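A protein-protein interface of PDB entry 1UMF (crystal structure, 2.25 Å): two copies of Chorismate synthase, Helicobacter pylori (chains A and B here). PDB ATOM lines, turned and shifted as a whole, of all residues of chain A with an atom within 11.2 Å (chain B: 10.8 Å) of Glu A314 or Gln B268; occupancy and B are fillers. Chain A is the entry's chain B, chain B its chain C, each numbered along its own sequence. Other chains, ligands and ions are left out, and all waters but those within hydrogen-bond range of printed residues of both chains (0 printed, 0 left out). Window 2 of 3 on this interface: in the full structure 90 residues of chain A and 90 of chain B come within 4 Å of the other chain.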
ATOM      1  N   ILE A  96      28.763  16.044  30.147  1.00  0.00           N
ATOM      2  CA  ILE A  96      29.469  17.202  30.716  1.00  0.00           C
ATOM      3  C   ILE A  96      28.568  17.909  31.733  1.00  0.00           C
ATOM      4  O   ILE A  96      27.588  18.549  31.356  1.00  0.00           O
ATOM      5  CB  ILE A  96      29.857  18.171  29.598  1.00  0.00           C
ATOM      6  N   ASN A  98      28.787  20.548  33.211  1.00  0.00           N
ATOM      7  CA  ASN A  98      29.165  21.955  33.283  1.00  0.00           C
ATOM      8  C   ASN A  98      28.084  22.832  32.663  1.00  0.00           C
ATOM      9  O   ASN A  98      28.361  23.924  32.169  1.00  0.00           O
ATOM     10  CB  ASN A  98      30.496  22.181  32.559  1.00  0.00           C
ATOM     11  CG  ASN A  98      31.654  21.455  33.224  1.00  0.00           C
ATOM     12  OD1 ASN A  98      31.991  21.724  34.379  1.00  0.00           O
ATOM     13  ND2 ASN A  98      32.268  20.526  32.496  1.00  0.00           N
ATOM     14  N   LEU A  99      26.849  22.343  32.693  1.00  0.00           N
ATOM     15  CA  LEU A  99      25.720  23.080  32.141  1.00  0.00           C
ATOM     16  C   LEU A  99      24.579  23.179  33.155  1.00  0.00           C
ATOM     17  O   LEU A  99      24.520  22.413  34.118  1.00  0.00           O
ATOM     18  CB  LEU A  99      25.236  22.408  30.848  1.00  0.00           C
ATOM     19  CG  LEU A  99      24.871  20.919  30.857  1.00  0.00           C
ATOM     20  CD1 LEU A  99      23.577  20.692  31.625  1.00  0.00           C
ATOM     21  CD2 LEU A  99      24.717  20.438  29.425  1.00  0.00           C
ATOM     22  N   PHE A 100      23.677  24.128  32.933  1.00  0.00           N
ATOM     23  CA  PHE A 100      22.547  24.332  33.831  1.00  0.00           C
ATOM     24  C   PHE A 100      21.339  23.500  33.402  1.00  0.00           C
ATOM     25  O   PHE A 100      20.773  23.717  32.330  1.00  0.00           O
ATOM     26  CB  PHE A 100      22.162  25.814  33.855  1.00  0.00           C
ATOM     27  CG  PHE A 100      23.340  26.747  33.939  1.00  0.00           C
ATOM     28  CD1 PHE A 100      24.227  26.678  35.011  1.00  0.00           C
ATOM     29  CD2 PHE A 100      23.565  27.689  32.938  1.00  0.00           C
ATOM     30  CE1 PHE A 100      25.326  27.537  35.085  1.00  0.00           C
ATOM     31  CE2 PHE A 100      24.659  28.554  33.000  1.00  0.00           C
ATOM     32  CZ  PHE A 100      25.542  28.478  34.076  1.00  0.00           C
ATOM     33  N   PRO A 102      17.659  22.505  33.037  1.00  0.00           N
ATOM     34  CA  PRO A 102      16.386  23.231  33.071  1.00  0.00           C
ATOM     35  C   PRO A 102      15.578  22.949  34.341  1.00  0.00           C
ATOM     36  O   PRO A 102      15.539  21.815  34.825  1.00  0.00           O
ATOM     37  CB  PRO A 102      15.687  22.744  31.804  1.00  0.00           C
ATOM     38  CG  PRO A 102      16.838  22.578  30.854  1.00  0.00           C
ATOM     39  CD  PRO A 102      17.871  21.877  31.718  1.00  0.00           C
ATOM     40  N   PHE A 107      21.646  27.122  37.737  1.00  0.00           N
ATOM     41  CA  PHE A 107      21.820  28.474  37.222  1.00  0.00           C
ATOM     42  C   PHE A 107      21.917  29.550  38.305  1.00  0.00           C
ATOM     43  O   PHE A 107      22.829  30.376  38.290  1.00  0.00           O
ATOM     44  CB  PHE A 107      20.673  28.820  36.271  1.00  0.00           C
ATOM     45  CG  PHE A 107      20.781  30.192  35.679  1.00  0.00           C
ATOM     46  CD1 PHE A 107      21.752  30.470  34.718  1.00  0.00           C
ATOM     47  CD2 PHE A 107      19.939  31.216  36.106  1.00  0.00           C
ATOM     48  CE1 PHE A 107      21.884  31.754  34.187  1.00  0.00           C
ATOM     49  CE2 PHE A 107      20.062  32.507  35.582  1.00  0.00           C
ATOM     50  CZ  PHE A 107      21.037  32.775  34.619  1.00  0.00           C
ATOM     51  N   HIS A 111      25.255  31.732  39.802  1.00  0.00           N
ATOM     52  CA  HIS A 111      25.366  33.181  39.841  1.00  0.00           C
ATOM     53  C   HIS A 111      25.457  33.759  41.249  1.00  0.00           C
ATOM     54  O   HIS A 111      26.191  34.719  41.477  1.00  0.00           O
ATOM     55  CB  HIS A 111      24.197  33.834  39.104  1.00  0.00           C
ATOM     56  CG  HIS A 111      24.395  33.920  37.622  1.00  0.00           C
ATOM     57  ND1 HIS A 111      24.240  32.838  36.784  1.00  0.00           N
ATOM     58  CD2 HIS A 111      24.752  34.960  36.833  1.00  0.00           C
ATOM     59  CE1 HIS A 111      24.492  33.207  35.541  1.00  0.00           C
ATOM     60  NE2 HIS A 111      24.804  34.490  35.543  1.00  0.00           N
ATOM     61  N   GLN A 305      16.950  18.723  26.173  1.00  0.00           N
ATOM     62  CA  GLN A 305      16.479  20.073  26.445  1.00  0.00           C
ATOM     63  C   GLN A 305      17.543  21.091  26.050  1.00  0.00           C
ATOM     64  O   GLN A 305      18.739  20.843  26.201  1.00  0.00           O
ATOM     65  CB  GLN A 305      16.156  20.233  27.934  1.00  0.00           C
ATOM     66  CG  GLN A 305      15.249  19.156  28.507  1.00  0.00           C
ATOM     67  CD  GLN A 305      14.925  19.379  29.979  1.00  0.00           C
ATOM     68  OE1 GLN A 305      14.199  20.309  30.336  1.00  0.00           O
ATOM     69  NE2 GLN A 305      15.469  18.524  30.841  1.00  0.00           N
ATOM     70  N   ARG A 306      17.103  22.234  25.535  1.00  0.00           N
ATOM     71  CA  ARG A 306      18.026  23.293  25.148  1.00  0.00           C
ATOM     72  C   ARG A 306      18.441  24.060  26.397  1.00  0.00           C
ATOM     73  O   ARG A 306      17.616  24.336  27.268  1.00  0.00           O
ATOM     74  CB  ARG A 306      17.361  24.267  24.175  1.00  0.00           C
ATOM     75  CG  ARG A 306      17.003  23.691  22.825  1.00  0.00           C
ATOM     76  CD  ARG A 306      16.338  24.766  21.987  1.00  0.00           C
ATOM     77  NE  ARG A 306      15.948  24.291  20.665  1.00  0.00           N
ATOM     78  CZ  ARG A 306      15.283  25.028  19.783  1.00  0.00           C
ATOM     79  NH1 ARG A 306      14.935  26.272  20.087  1.00  0.00           N
ATOM     80  NH2 ARG A 306      14.967  24.523  18.598  1.00  0.00           N
ATOM     81  N   THR A 307      19.719  24.406  26.479  1.00  0.00           N
ATOM     82  CA  THR A 307      20.232  25.147  27.623  1.00  0.00           C
ATOM     83  C   THR A 307      21.674  25.557  27.365  1.00  0.00           C
ATOM     84  O   THR A 307      22.282  25.128  26.385  1.00  0.00           O
ATOM     85  CB  THR A 307      20.166  24.297  28.908  1.00  0.00           C
ATOM     86  OG1 THR A 307      20.536  25.103  30.032  1.00  0.00           O
ATOM     87  CG2 THR A 307      21.106  23.102  28.808  1.00  0.00           C
ATOM     88  N   ILE A 308      22.220  26.395  28.241  1.00  0.00           N
ATOM     89  CA  ILE A 308      23.594  26.858  28.094  1.00  0.00           C
ATOM     90  C   ILE A 308      24.491  26.200  29.132  1.00  0.00           C
ATOM     91  O   ILE A 308      24.020  25.448  29.984  1.00  0.00           O
ATOM     92  CB  ILE A 308      23.695  28.394  28.262  1.00  0.00           C
ATOM     93  CG1 ILE A 308      23.324  28.792  29.692  1.00  0.00           C
ATOM     94  CG2 ILE A 308      22.772  29.088  27.269  1.00  0.00           C
ATOM     95  CD1 ILE A 308      23.494  30.270  29.984  1.00  0.00           C
ATOM     96  N   ASP A 309      25.786  26.484  29.052  1.00  0.00           N
ATOM     97  CA  ASP A 309      26.747  25.934  29.997  1.00  0.00           C
ATOM     98  C   ASP A 309      27.397  27.073  30.780  1.00  0.00           C
ATOM     99  O   ASP A 309      27.140  28.248  30.509  1.00  0.00           O
ATOM    100  CB  ASP A 309      27.807  25.104  29.261  1.00  0.00           C
ATOM    101  CG  ASP A 309      28.612  25.922  28.270  1.00  0.00           C
ATOM    102  OD1 ASP A 309      28.008  26.583  27.403  1.00  0.00           O
ATOM    103  OD2 ASP A 309      29.857  25.895  28.356  1.00  0.00           O
ATOM    104  N   ILE A 310      28.233  26.721  31.751  1.00  0.00           N
ATOM    105  CA  ILE A 310      28.914  27.700  32.592  1.00  0.00           C
ATOM    106  C   ILE A 310      29.579  28.832  31.806  1.00  0.00           C
ATOM    107  O   ILE A 310      29.904  29.880  32.371  1.00  0.00           O
ATOM    108  CB  ILE A 310      29.976  27.010  33.480  1.00  0.00           C
ATOM    109  CG1 ILE A 310      29.312  25.923  34.328  1.00  0.00           C
ATOM    110  CG2 ILE A 310      30.643  28.025  34.394  1.00  0.00           C
ATOM    111  CD1 ILE A 310      30.281  25.134  35.185  1.00  0.00           C
ATOM    112  N   ASN A 311      29.770  28.633  30.505  1.00  0.00           N
ATOM    113  CA  ASN A 311      30.405  29.648  29.671  1.00  0.00           C
ATOM    114  C   ASN A 311      29.445  30.417  28.767  1.00  0.00           C
ATOM    115  O   ASN A 311      29.825  31.429  28.180  1.00  0.00           O
ATOM    116  CB  ASN A 311      31.518  29.017  28.832  1.00  0.00           C
ATOM    117  CG  ASN A 311      32.683  28.544  29.682  1.00  0.00           C
ATOM    118  OD1 ASN A 311      33.277  29.326  30.427  1.00  0.00           O
ATOM    119  ND2 ASN A 311      33.015  27.261  29.575  1.00  0.00           N
ATOM    120  N   GLY A 312      28.211  29.939  28.648  1.00  0.00           N
ATOM    121  CA  GLY A 312      27.236  30.635  27.825  1.00  0.00           C
ATOM    122  C   GLY A 312      26.832  29.962  26.526  1.00  0.00           C
ATOM    123  O   GLY A 312      25.692  30.101  26.083  1.00  0.00           O
ATOM    124  N   ASN A 313      27.761  29.241  25.909  1.00  0.00           N
ATOM    125  CA  ASN A 313      27.489  28.552  24.649  1.00  0.00           C
ATOM    126  C   ASN A 313      26.251  27.661  24.764  1.00  0.00           C
ATOM    127  O   ASN A 313      25.983  27.095  25.825  1.00  0.00           O
ATOM    128  CB  ASN A 313      28.700  27.706  24.248  1.00  0.00           C
ATOM    129  CG  ASN A 313      29.961  28.536  24.071  1.00  0.00           C
ATOM    130  OD1 ASN A 313      31.065  27.998  23.983  1.00  0.00           O
ATOM    131  ND2 ASN A 313      29.801  29.854  24.011  1.00  0.00           N
ATOM    132  N   GLU A 314      25.497  27.541  23.676  1.00  0.00           N
ATOM    133  CA  GLU A 314      24.301  26.705  23.674  1.00  0.00           C
ATOM    134  C   GLU A 314      24.701  25.237  23.584  1.00  0.00           C
ATOM    135  O   GLU A 314      25.575  24.877  22.798  1.00  0.00           O
ATOM    136  CB  GLU A 314      23.401  27.049  22.487  1.00  0.00           C
ATOM    137  CG  GLU A 314      22.914  28.487  22.447  1.00  0.00           C
ATOM    138  CD  GLU A 314      21.892  28.715  21.349  1.00  0.00           C
ATOM    139  OE1 GLU A 314      21.470  29.872  21.158  1.00  0.00           O
ATOM    140  OE2 GLU A 314      21.508  27.736  20.678  1.00  0.00           O
ATOM    141  N   CYS A 315      24.058  24.395  24.387  1.00  0.00           N
ATOM    142  CA  CYS A 315      24.349  22.966  24.387  1.00  0.00           C
ATOM    143  C   CYS A 315      23.108  22.140  24.729  1.00  0.00           C
ATOM    144  O   CYS A 315      22.089  22.682  25.164  1.00  0.00           O
ATOM    145  CB  CYS A 315      25.473  22.655  25.378  1.00  0.00           C
ATOM    146  SG  CYS A 315      25.142  23.176  27.070  1.00  0.00           S
ATOM    147  N   GLU A 316      23.201  20.829  24.528  1.00  0.00           N
ATOM    148  CA  GLU A 316      22.083  19.932  24.797  1.00  0.00           C
ATOM    149  C   GLU A 316      22.201  19.196  26.123  1.00  0.00           C
ATOM    150  O   GLU A 316      23.209  18.550  26.401  1.00  0.00           O
ATOM    151  CB  GLU A 316      21.940  18.909  23.665  1.00  0.00           C
ATOM    152  CG  GLU A 316      21.010  17.748  23.995  1.00  0.00           C
ATOM    153  CD  GLU A 316      20.912  16.731  22.873  1.00  0.00           C
ATOM    154  OE1 GLU A 316      20.302  15.663  23.090  1.00  0.00           O
ATOM    155  OE2 GLU A 316      21.438  16.999  21.771  1.00  0.00           O
ATOM    156  N   CYS A 317      21.155  19.298  26.935  1.00  0.00           N
ATOM    157  CA  CYS A 317      21.122  18.630  28.228  1.00  0.00           C
ATOM    158  C   CYS A 317      20.338  17.330  28.093  1.00  0.00           C
ATOM    159  O   CYS A 317      19.129  17.341  27.845  1.00  0.00           O
ATOM    160  CB  CYS A 317      20.463  19.526  29.283  1.00  0.00           C
ATOM    161  SG  CYS A 317      20.288  18.762  30.921  1.00  0.00           S
ATOM    162  N   LEU A 318      21.037  16.212  28.245  1.00  0.00           N
ATOM    163  CA  LEU A 318      20.411  14.903  28.146  1.00  0.00           C
ATOM    164  C   LEU A 318      20.684  14.159  29.447  1.00  0.00           C
ATOM    165  O   LEU A 318      21.797  13.687  29.681  1.00  0.00           O
ATOM    166  CB  LEU A 318      20.989  14.140  26.946  1.00  0.00           C
ATOM    167  CG  LEU A 318      20.340  12.822  26.503  1.00  0.00           C
ATOM    168  CD1 LEU A 318      20.616  11.738  27.528  1.00  0.00           C
ATOM    169  CD2 LEU A 318      18.841  13.018  26.304  1.00  0.00           C
ATOM    170  N   LYS B 216      17.626  42.301  32.840  1.00  0.00           N
ATOM    171  CA  LYS B 216      17.447  41.220  33.805  1.00  0.00           C
ATOM    172  C   LYS B 216      17.615  41.681  35.246  1.00  0.00           C
ATOM    173  O   LYS B 216      18.356  42.623  35.521  1.00  0.00           O
ATOM    174  CB  LYS B 216      18.453  40.093  33.524  1.00  0.00           C
ATOM    175  CG  LYS B 216      18.371  39.483  32.126  1.00  0.00           C
ATOM    176  CD  LYS B 216      17.041  38.782  31.902  1.00  0.00           C
ATOM    177  CE  LYS B 216      16.938  38.220  30.496  1.00  0.00           C
ATOM    178  NZ  LYS B 216      15.600  37.616  30.250  1.00  0.00           N
ATOM    179  N   LEU B 265      13.450  26.494  29.142  1.00  0.00           N
ATOM    180  CA  LEU B 265      14.681  26.292  28.391  1.00  0.00           C
ATOM    181  C   LEU B 265      15.441  27.612  28.307  1.00  0.00           C
ATOM    182  O   LEU B 265      14.852  28.688  28.432  1.00  0.00           O
ATOM    183  CB  LEU B 265      14.368  25.772  26.982  1.00  0.00           C
ATOM    184  CG  LEU B 265      13.635  24.429  26.839  1.00  0.00           C
ATOM    185  CD1 LEU B 265      14.363  23.352  27.640  1.00  0.00           C
ATOM    186  CD2 LEU B 265      12.195  24.566  27.322  1.00  0.00           C
ATOM    187  N   MET B 266      16.750  27.530  28.096  1.00  0.00           N
ATOM    188  CA  MET B 266      17.574  28.726  28.010  1.00  0.00           C
ATOM    189  C   MET B 266      18.072  29.021  26.598  1.00  0.00           C
ATOM    190  O   MET B 266      18.425  28.113  25.846  1.00  0.00           O
ATOM    191  CB  MET B 266      18.752  28.610  28.979  1.00  0.00           C
ATOM    192  CG  MET B 266      18.326  28.706  30.439  1.00  0.00           C
ATOM    193  SD  MET B 266      19.689  28.613  31.610  1.00  0.00           S
ATOM    194  CE  MET B 266      19.391  27.002  32.342  1.00  0.00           C
ATOM    195  N   ASP B 267      18.092  30.307  26.254  1.00  0.00           N
ATOM    196  CA  ASP B 267      18.520  30.774  24.937  1.00  0.00           C
ATOM    197  C   ASP B 267      19.964  31.284  24.968  1.00  0.00           C
ATOM    198  O   ASP B 267      20.759  30.864  25.809  1.00  0.00           O
ATOM    199  CB  ASP B 267      17.582  31.893  24.470  1.00  0.00           C
ATOM    200  CG  ASP B 267      17.636  32.120  22.974  1.00  0.00           C
ATOM    201  OD1 ASP B 267      16.905  33.009  22.482  1.00  0.00           O
ATOM    202  OD2 ASP B 267      18.404  31.409  22.291  1.00  0.00           O
ATOM    203  N   GLN B 268      20.297  32.190  24.051  1.00  0.00           N
ATOM    204  CA  GLN B 268      21.644  32.752  23.987  1.00  0.00           C
ATOM    205  C   GLN B 268      21.919  33.650  25.186  1.00  0.00           C
ATOM    206  O   GLN B 268      23.035  33.680  25.704  1.00  0.00           O
ATOM    207  CB  GLN B 268      21.834  33.550  22.694  1.00  0.00           C
ATOM    208  CG  GLN B 268      21.791  32.702  21.438  1.00  0.00           C
ATOM    209  CD  GLN B 268      22.152  33.484  20.193  1.00  0.00           C
ATOM    210  OE1 GLN B 268      23.244  34.046  20.093  1.00  0.00           O
ATOM    211  NE2 GLN B 268      21.238  33.522  19.230  1.00  0.00           N
ATOM    212  N   LYS B 269      20.897  34.383  25.617  1.00  0.00           N
ATOM    213  CA  LYS B 269      21.015  35.275  26.768  1.00  0.00           C
ATOM    214  C   LYS B 269      19.677  35.442  27.483  1.00  0.00           C
ATOM    215  O   LYS B 269      19.011  36.470  27.351  1.00  0.00           O
ATOM    216  CB  LYS B 269      21.550  36.648  26.339  1.00  0.00           C
ATOM    217  CG  LYS B 269      23.023  36.653  25.956  1.00  0.00           C
ATOM    218  CD  LYS B 269      23.528  38.063  25.689  1.00  0.00           C
ATOM    219  CE  LYS B 269      25.025  38.069  25.416  1.00  0.00           C
ATOM    220  NZ  LYS B 269      25.550  39.449  25.225  1.00  0.00           N
ATOM    221  N   GLY B 270      19.292  34.421  28.243  1.00  0.00           N
ATOM    222  CA  GLY B 270      18.037  34.470  28.972  1.00  0.00           C
ATOM    223  C   GLY B 270      17.215  33.207  28.805  1.00  0.00           C
ATOM    224  O   GLY B 270      17.576  32.316  28.032  1.00  0.00           O
ATOM    225  N   PHE B 271      16.107  33.129  29.534  1.00  0.00           N
ATOM    226  CA  PHE B 271      15.223  31.972  29.465  1.00  0.00           C
ATOM    227  C   PHE B 271      14.180  32.161  28.366  1.00  0.00           C
ATOM    228  O   PHE B 271      13.671  33.262  28.166  1.00  0.00           O
ATOM    229  CB  PHE B 271      14.524  31.755  30.813  1.00  0.00           C
ATOM    230  CG  PHE B 271      15.466  31.463  31.947  1.00  0.00           C
ATOM    231  CD1 PHE B 271      16.197  32.487  32.547  1.00  0.00           C
ATOM    232  CD2 PHE B 271      15.634  30.160  32.412  1.00  0.00           C
ATOM    233  CE1 PHE B 271      17.081  32.214  33.594  1.00  0.00           C
ATOM    234  CE2 PHE B 271      16.511  29.878  33.455  1.00  0.00           C
ATOM    235  CZ  PHE B 271      17.236  30.906  34.048  1.00  0.00           C
ATOM    236  N   LEU B 272      13.867  31.083  27.656  1.00  0.00           N
ATOM    237  CA  LEU B 272      12.887  31.140  26.577  1.00  0.00           C
ATOM    238  C   LEU B 272      11.461  31.285  27.115  1.00  0.00           C
ATOM    239  O   LEU B 272      10.530  31.570  26.359  1.00  0.00           O
ATOM    240  CB  LEU B 272      13.003  29.885  25.705  1.00  0.00           C
ATOM    241  CG  LEU B 272      14.358  29.707  25.014  1.00  0.00           C
ATOM    242  CD1 LEU B 272      14.458  28.324  24.395  1.00  0.00           C
ATOM    243  CD2 LEU B 272      14.528  30.785  23.957  1.00  0.00           C
ATOM    244  N   SER B 273      11.299  31.087  28.422  1.00  0.00           N
ATOM    245  CA  SER B 273       9.997  31.207  29.076  1.00  0.00           C
ATOM    246  C   SER B 273      10.195  31.454  30.572  1.00  0.00           C
ATOM    247  O   SER B 273      11.281  31.213  31.110  1.00  0.00           O
ATOM    248  CB  SER B 273       9.171  29.937  28.861  1.00  0.00           C
ATOM    249  OG  SER B 273       9.876  28.788  29.290  1.00  0.00           O
ATOM    250  N   GLU B 287      14.619  36.689  35.555  1.00  0.00           N
ATOM    251  CA  GLU B 287      13.396  37.012  34.836  1.00  0.00           C
ATOM    252  C   GLU B 287      12.426  37.704  35.782  1.00  0.00           C
ATOM    253  O   GLU B 287      12.688  37.803  36.987  1.00  0.00           O
ATOM    254  CB  GLU B 287      12.774  35.741  34.255  1.00  0.00           C
ATOM    255  CG  GLU B 287      13.726  34.986  33.334  1.00  0.00           C
ATOM    256  CD  GLU B 287      14.253  35.849  32.192  1.00  0.00           C
ATOM    257  OE1 GLU B 287      15.420  35.660  31.795  1.00  0.00           O
ATOM    258  OE2 GLU B 287      13.504  36.709  31.681  1.00  0.00           O
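O of Ile A308 sits at hydrogen-bond distance from N of Phe A100 (3.2 Å). O of Thr A307 sits at hydrogen-bond distance from N of Cys A315, 2.8 Å away. The backbone carbonyl oxygen (O) of Leu B265 sits at hydrogen-bond distance from the backbone NH (N) of Leu B272, 2.7 Å away. The backbone carbonyl oxygen of Gln A305 is in hydrogen-bond range of the backbone NH of Cys A317. ND1 of His A111 is in hydrogen-bond range of O of Phe A107 (3.2 Å). The side-chain carboxylate (OE1) of Glu B287 lies close to the backbone NH (N) of Phe B271 (3.5 Å).
Among the printed residues, merely in contact across the chains: Phe A100 with Met B266 (3.4 Å), Phe A107 with Phe B271 (3.4 Å), Gln A305 with Leu B265 (3.6 Å), Arg A306 with Leu B265 (3.4 Å), Thr A307 with Met B266 (3.2 Å), Ile A308 with Asp B267 (3.1 Å), Glu A314 with Asp B267 (3.6 Å) and Glu A314 with Gln B268 (2.9 Å).
Asp A309 touches none of the printed residues of chain B. No residue of chain B comes within 4 Å of Gly A312. No residue of chain B comes within 4 Å of Asn A313. Of the printed residues of chain B, Glu A314 touches Asp B267 (3.6 Å) and Gln B268 (2.9 Å). Leu A318 touches none of the printed residues of chain B. Of the printed residues of chain A, Leu B265 touches Gln A305 (3.6 Å) and Arg A306 (3.4 Å). Printed residues of chain A within 4 Å of Met B266: Phe A100, Arg A306 and Thr A307. Printed residues of chain A within 4 Å of Asp B267: Ile A308 (3.1 Å) and Glu A314 (3.6 Å). No residue of chain A comes within 4 Å of Lys B269. Gly B270 touches none of the printed residues of chain A. The nearest residue of chain A that does not touch Gln B268 is Gly A312 (4.5 Å). The nearest printed residue of chain B that does not touch Arg A306 is Leu B272 (4.7 Å).
No position is printed for both chains. Of the 9 pairs that touch across the chains among the printed residues, none has its exchanged pair printed and touching as well.
O of Arg A306 lies within hydrogen-bond range of N of Met B266, at 3.4 Å.
Hydrophobic or aromatic side chains of chain A within 4 Å of the printed part of chain B: Phe A100, Phe A107 and Ile A308. Along chain A the printed residues that touch a printed residue of chain B span positions 100 to 314. Of the 11 printed residues of chain B, 5 touch a printed residue of chain A. Printed residues of chain B that touch a printed residue of chain A: Leu B265, Met B266, Asp B267, Gln B268 and Phe B271. Among the printed residues, no Asp or Glu carboxylate lies within 4 Å of a Lys or Arg side-chain nitrogen of the other chain.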
